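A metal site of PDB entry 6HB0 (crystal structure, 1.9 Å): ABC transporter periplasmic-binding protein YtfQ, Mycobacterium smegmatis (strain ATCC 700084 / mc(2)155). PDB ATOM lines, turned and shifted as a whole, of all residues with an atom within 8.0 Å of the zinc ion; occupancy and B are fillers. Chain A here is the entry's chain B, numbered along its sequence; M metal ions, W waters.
Merely in contact with the zinc ion: Thr 290. Within 4 Å of the zinc ion: Glu 128, Cys 263, Thr 290 and Asp 292.
The zinc ion is bound by OD1 of Asp 292 (2.0 Å), water W1 (2.0 Å), OE1 of Glu 128 (2.0 Å) and SG of Cys 263 (2.2 Å). Slightly farther from the zinc ion lies OE2 of Glu 128 (2.8 Å).
The guanidinium group (NH1) of Arg 132 is in salt-bridge range of the side-chain carboxylate (OE2) of Glu 128, 2.9 Å away. The backbone NH (N) of Cys 263 is in hydrogen-bond range of the side-chain carboxylate (OE2) of Glu 129 (2.8 Å). OG1 of Thr 290 is in hydrogen-bond range of O of Asn 264 (2.6 Å). The side-chain sulfur of Cys 263 lies close to the side-chain hydroxyl of Thr 290 (3.3 Å). The side-chain sulfur (SG) of Cys 263 sits close to the backbone NH (N) of Asp 125 (3.3 Å). OD1 of Asp 125 is in hydrogen-bond range of N of Glu 128 (3.2 Å). The side-chain carboxylate (OD1) of Asp 292 sits close to the guanidinium group (NH1) of Arg 132 (3.5 Å).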
ATOM      1  N   GLY A 123     -14.964  13.659  15.882  1.00  0.00           N
ATOM      2  CA  GLY A 123     -14.039  14.180  16.892  1.00  0.00           C
ATOM      3  C   GLY A 123     -12.857  13.240  17.047  1.00  0.00           C
ATOM      4  O   GLY A 123     -12.779  12.202  16.368  1.00  0.00           O
ATOM      5  N   ALA A 124     -11.912  13.646  17.888  1.00  0.00           N
ATOM      6  CA  ALA A 124     -10.719  12.852  18.088  1.00  0.00           C
ATOM      7  C   ALA A 124     -11.133  11.640  18.903  1.00  0.00           C
ATOM      8  O   ALA A 124     -12.008  11.732  19.739  1.00  0.00           O
ATOM      9  CB  ALA A 124      -9.662  13.650  18.802  1.00  0.00           C
ATOM     10  N   ASP A 125     -10.473  10.543  18.637  1.00  0.00           N
ATOM     11  CA  ASP A 125     -10.534   9.305  19.415  1.00  0.00           C
ATOM     12  C   ASP A 125      -9.337   9.215  20.401  1.00  0.00           C
ATOM     13  O   ASP A 125      -8.249   8.842  20.021  1.00  0.00           O
ATOM     14  CB  ASP A 125     -10.452   8.164  18.437  1.00  0.00           C
ATOM     15  CG  ASP A 125     -10.683   6.785  19.095  1.00  0.00           C
ATOM     16  OD1 ASP A 125     -10.662   6.660  20.361  1.00  0.00           O
ATOM     17  OD2 ASP A 125     -10.901   5.861  18.293  1.00  0.00           O
ATOM     18  N   PHE A 126      -9.575   9.582  21.646  1.00  0.00           N
ATOM     19  CA  PHE A 126      -8.537   9.702  22.628  1.00  0.00           C
ATOM     20  C   PHE A 126      -8.032   8.311  23.071  1.00  0.00           C
ATOM     21  O   PHE A 126      -6.890   8.181  23.409  1.00  0.00           O
ATOM     22  CB  PHE A 126      -9.069  10.440  23.841  1.00  0.00           C
ATOM     23  CG  PHE A 126      -9.625  11.801  23.531  1.00  0.00           C
ATOM     24  CD1 PHE A 126      -8.871  12.727  22.854  1.00  0.00           C
ATOM     25  CD2 PHE A 126     -10.932  12.150  23.937  1.00  0.00           C
ATOM     26  CE1 PHE A 126      -9.373  13.996  22.575  1.00  0.00           C
ATOM     27  CE2 PHE A 126     -11.462  13.408  23.629  1.00  0.00           C
ATOM     28  CZ  PHE A 126     -10.673  14.320  22.954  1.00  0.00           C
ATOM     29  N   ILE A 127      -8.885   7.298  23.058  1.00  0.00           N
ATOM     30  CA  ILE A 127      -8.432   5.904  23.346  1.00  0.00           C
ATOM     31  C   ILE A 127      -7.423   5.512  22.318  1.00  0.00           C
ATOM     32  O   ILE A 127      -6.342   5.029  22.635  1.00  0.00           O
ATOM     33  CB  ILE A 127      -9.585   4.890  23.373  1.00  0.00           C
ATOM     34  CG1 ILE A 127     -10.536   5.256  24.507  1.00  0.00           C
ATOM     35  CG2 ILE A 127      -9.021   3.471  23.480  1.00  0.00           C
ATOM     36  CD1 ILE A 127     -11.634   4.236  24.821  1.00  0.00           C
ATOM     37  N   GLU A 128      -7.727   5.763  21.071  1.00  0.00           N
ATOM     38  CA  GLU A 128      -6.835   5.416  19.979  1.00  0.00           C
ATOM     39  C   GLU A 128      -5.511   6.150  20.116  1.00  0.00           C
ATOM     40  O   GLU A 128      -4.460   5.594  19.837  1.00  0.00           O
ATOM     41  CB  GLU A 128      -7.502   5.759  18.649  1.00  0.00           C
ATOM     42  CG  GLU A 128      -6.684   5.554  17.415  1.00  0.00           C
ATOM     43  CD  GLU A 128      -6.602   6.852  16.635  1.00  0.00           C
ATOM     44  OE1 GLU A 128      -7.465   7.081  15.780  1.00  0.00           O
ATOM     45  OE2 GLU A 128      -5.681   7.655  16.883  1.00  0.00           O
ATOM     46  N   GLU A 129      -5.527   7.409  20.566  1.00  0.00           N
ATOM     47  CA  GLU A 129      -4.242   8.136  20.795  1.00  0.00           C
ATOM     48  C   GLU A 129      -3.388   7.418  21.801  1.00  0.00           C
ATOM     49  O   GLU A 129      -2.212   7.213  21.576  1.00  0.00           O
ATOM     50  CB  GLU A 129      -4.449   9.579  21.328  1.00  0.00           C
ATOM     51  CG  GLU A 129      -4.960  10.529  20.285  1.00  0.00           C
ATOM     52  CD  GLU A 129      -5.211  11.961  20.784  1.00  0.00           C
ATOM     53  OE1 GLU A 129      -5.792  12.095  21.873  1.00  0.00           O
ATOM     54  OE2 GLU A 129      -4.874  12.948  20.037  1.00  0.00           O
ATOM     55  N   ARG A 131      -3.616   4.336  22.724  1.00  0.00           N
ATOM     56  CA  ARG A 131      -3.190   3.072  22.164  1.00  0.00           C
ATOM     57  C   ARG A 131      -2.007   3.168  21.245  1.00  0.00           C
ATOM     58  O   ARG A 131      -1.096   2.336  21.290  1.00  0.00           O
ATOM     59  CB  ARG A 131      -4.353   2.393  21.417  1.00  0.00           C
ATOM     60  CG  ARG A 131      -4.022   0.982  20.957  1.00  0.00           C
ATOM     61  CD  ARG A 131      -5.287   0.222  20.616  1.00  0.00           C
ATOM     62  NE  ARG A 131      -5.855   0.871  19.502  1.00  0.00           N
ATOM     63  CZ  ARG A 131      -7.073   1.363  19.373  1.00  0.00           C
ATOM     64  NH1 ARG A 131      -8.050   1.157  20.227  1.00  0.00           N
ATOM     65  NH2 ARG A 131      -7.285   1.995  18.251  1.00  0.00           N
ATOM     66  N   ARG A 132      -2.000   4.151  20.373  1.00  0.00           N
ATOM     67  CA  ARG A 132      -0.854   4.314  19.487  1.00  0.00           C
ATOM     68  C   ARG A 132       0.432   4.714  20.251  1.00  0.00           C
ATOM     69  O   ARG A 132       1.532   4.283  19.904  1.00  0.00           O
ATOM     70  CB  ARG A 132      -1.208   5.286  18.365  1.00  0.00           C
ATOM     71  CG  ARG A 132      -2.323   4.780  17.431  1.00  0.00           C
ATOM     72  CD  ARG A 132      -3.121   5.934  16.767  1.00  0.00           C
ATOM     73  NE  ARG A 132      -2.169   6.737  16.119  1.00  0.00           N
ATOM     74  CZ  ARG A 132      -2.119   8.047  15.992  1.00  0.00           C
ATOM     75  NH1 ARG A 132      -3.092   8.869  16.348  1.00  0.00           N
ATOM     76  NH2 ARG A 132      -1.035   8.506  15.423  1.00  0.00           N
ATOM     77  N   GLU A 262      -1.049  12.085  17.486  1.00  0.00           N
ATOM     78  CA  GLU A 262      -2.249  12.916  17.629  1.00  0.00           C
ATOM     79  C   GLU A 262      -3.339  12.328  16.807  1.00  0.00           C
ATOM     80  O   GLU A 262      -3.078  11.834  15.755  1.00  0.00           O
ATOM     81  CB  GLU A 262      -1.999  14.364  17.205  1.00  0.00           C
ATOM     82  CG  GLU A 262      -3.206  15.228  17.479  1.00  0.00           C
ATOM     83  CD  GLU A 262      -3.041  16.709  17.125  1.00  0.00           C
ATOM     84  OE1 GLU A 262      -1.926  17.262  17.189  1.00  0.00           O
ATOM     85  OE2 GLU A 262      -4.078  17.312  16.862  1.00  0.00           O
ATOM     86  N   CYS A 263      -4.564  12.347  17.344  1.00  0.00           N
ATOM     87  CA  CYS A 263      -5.753  12.053  16.571  1.00  0.00           C
ATOM     88  C   CYS A 263      -6.396  13.405  16.376  1.00  0.00           C
ATOM     89  O   CYS A 263      -6.710  14.101  17.344  1.00  0.00           O
ATOM     90  CB  CYS A 263      -6.682  11.118  17.331  1.00  0.00           C
ATOM     91  SG  CYS A 263      -8.144  10.687  16.362  1.00  0.00           S
ATOM     92  N   ASN A 264      -6.577  13.815  15.119  1.00  0.00           N
ATOM     93  CA  ASN A 264      -7.110  15.163  14.852  1.00  0.00           C
ATOM     94  C   ASN A 264      -8.566  15.371  15.320  1.00  0.00           C
ATOM     95  O   ASN A 264      -9.381  14.451  15.355  1.00  0.00           O
ATOM     96  CB  ASN A 264      -7.103  15.463  13.349  1.00  0.00           C
ATOM     97  CG  ASN A 264      -5.700  15.677  12.765  1.00  0.00           C
ATOM     98  OD1 ASN A 264      -5.554  15.609  11.564  1.00  0.00           O
ATOM     99  ND2 ASN A 264      -4.696  15.950  13.595  1.00  0.00           N
ATOM    100  N   PRO A 265      -8.904  16.594  15.693  1.00  0.00           N
ATOM    101  CA  PRO A 265     -10.303  16.926  15.815  1.00  0.00           C
ATOM    102  C   PRO A 265     -10.989  17.020  14.432  1.00  0.00           C
ATOM    103  O   PRO A 265     -10.370  16.754  13.399  1.00  0.00           O
ATOM    104  CB  PRO A 265     -10.240  18.302  16.486  1.00  0.00           C
ATOM    105  CG  PRO A 265      -9.058  18.921  15.869  1.00  0.00           C
ATOM    106  CD  PRO A 265      -8.062  17.796  15.729  1.00  0.00           C
ATOM    107  N   ARG A 287     -19.101   7.168  13.586  1.00  0.00           N
ATOM    108  CA  ARG A 287     -17.972   7.975  13.989  1.00  0.00           C
ATOM    109  C   ARG A 287     -17.078   8.171  12.795  1.00  0.00           C
ATOM    110  O   ARG A 287     -16.665   7.223  12.175  1.00  0.00           O
ATOM    111  CB  ARG A 287     -17.188   7.231  15.027  1.00  0.00           C
ATOM    112  CG  ARG A 287     -17.467   7.653  16.443  1.00  0.00           C
ATOM    113  CD  ARG A 287     -16.248   8.440  16.887  1.00  0.00           C
ATOM    114  NE  ARG A 287     -15.960   8.267  18.283  1.00  0.00           N
ATOM    115  CZ  ARG A 287     -14.968   8.883  18.885  1.00  0.00           C
ATOM    116  NH1 ARG A 287     -14.796   8.637  20.152  1.00  0.00           N
ATOM    117  NH2 ARG A 287     -14.151   9.745  18.234  1.00  0.00           N
ATOM    118  N   VAL A 288     -16.840   9.395  12.421  1.00  0.00           N
ATOM    119  CA  VAL A 288     -15.901   9.648  11.371  1.00  0.00           C
ATOM    120  C   VAL A 288     -14.545   9.330  11.965  1.00  0.00           C
ATOM    121  O   VAL A 288     -14.282   9.637  13.134  1.00  0.00           O
ATOM    122  CB  VAL A 288     -15.982  11.109  10.969  1.00  0.00           C
ATOM    123  CG1 VAL A 288     -14.831  11.492  10.096  1.00  0.00           C
ATOM    124  CG2 VAL A 288     -17.230  11.336  10.179  1.00  0.00           C
ATOM    125  N   VAL A 289     -13.655   8.743  11.177  1.00  0.00           N
ATOM    126  CA  VAL A 289     -12.289   8.622  11.638  1.00  0.00           C
ATOM    127  C   VAL A 289     -11.490   9.820  11.111  1.00  0.00           C
ATOM    128  O   VAL A 289     -11.335   9.971   9.909  1.00  0.00           O
ATOM    129  CB  VAL A 289     -11.651   7.273  11.251  1.00  0.00           C
ATOM    130  CG1 VAL A 289     -12.559   6.103  11.718  1.00  0.00           C
ATOM    131  CG2 VAL A 289     -11.366   7.239   9.780  1.00  0.00           C
ATOM    132  N   THR A 290     -11.031  10.686  12.012  1.00  0.00           N
ATOM    133  CA  THR A 290     -10.273  11.873  11.627  1.00  0.00           C
ATOM    134  C   THR A 290      -8.859  11.434  11.275  1.00  0.00           C
ATOM    135  O   THR A 290      -8.497  10.289  11.533  1.00  0.00           O
ATOM    136  CB  THR A 290     -10.231  12.899  12.781  1.00  0.00           C
ATOM    137  OG1 THR A 290      -9.787  12.263  13.992  1.00  0.00           O
ATOM    138  CG2 THR A 290     -11.626  13.468  13.005  1.00  0.00           C
ATOM    139  N   PRO A 291      -8.079  12.289  10.643  1.00  0.00           N
ATOM    140  CA  PRO A 291      -6.699  11.901  10.353  1.00  0.00           C
ATOM    141  C   PRO A 291      -5.838  11.796  11.604  1.00  0.00           C
ATOM    142  O   PRO A 291      -6.089  12.473  12.649  1.00  0.00           O
ATOM    143  CB  PRO A 291      -6.186  13.040   9.457  1.00  0.00           C
ATOM    144  CG  PRO A 291      -7.416  13.634   8.903  1.00  0.00           C
ATOM    145  CD  PRO A 291      -8.419  13.568  10.013  1.00  0.00           C
ATOM    146  N   ASP A 292      -4.851  10.932  11.488  1.00  0.00           N
ATOM    147  CA  ASP A 292      -3.895  10.680  12.539  1.00  0.00           C
ATOM    148  C   ASP A 292      -2.526  11.186  12.155  1.00  0.00           C
ATOM    149  O   ASP A 292      -2.134  11.161  11.002  1.00  0.00           O
ATOM    150  CB  ASP A 292      -3.865   9.176  12.817  1.00  0.00           C
ATOM    151  CG  ASP A 292      -5.100   8.685  13.468  1.00  0.00           C
ATOM    152  OD1 ASP A 292      -5.767   9.452  14.215  1.00  0.00           O
ATOM    153  OD2 ASP A 292      -5.459   7.522  13.247  1.00  0.00           O
ATOM    154  N   GLU A 293      -1.822  11.696  13.139  1.00  0.00           N
ATOM    155  CA  GLU A 293      -0.469  12.190  12.993  1.00  0.00           C
ATOM    156  C   GLU A 293       0.441  11.384  13.920  1.00  0.00           C
ATOM    157  O   GLU A 293      -0.012  10.950  14.995  1.00  0.00           O
ATOM    158  CB  GLU A 293      -0.442  13.657  13.387  1.00  0.00           C
ATOM    159  CG  GLU A 293      -1.250  14.536  12.451  1.00  0.00           C
ATOM    160  CD  GLU A 293      -1.141  16.044  12.728  1.00  0.00           C
ATOM    161  OE1 GLU A 293      -0.033  16.553  13.019  1.00  0.00           O
ATOM    162  OE2 GLU A 293      -2.162  16.733  12.609  1.00  0.00           O
HETATM  163 ZN    ZN M   1      -7.434   9.023  15.161  1.00  0.00          ZN
HETATM  164  O   HOH W   1      -8.792   8.612  13.707  1.00  0.00           O
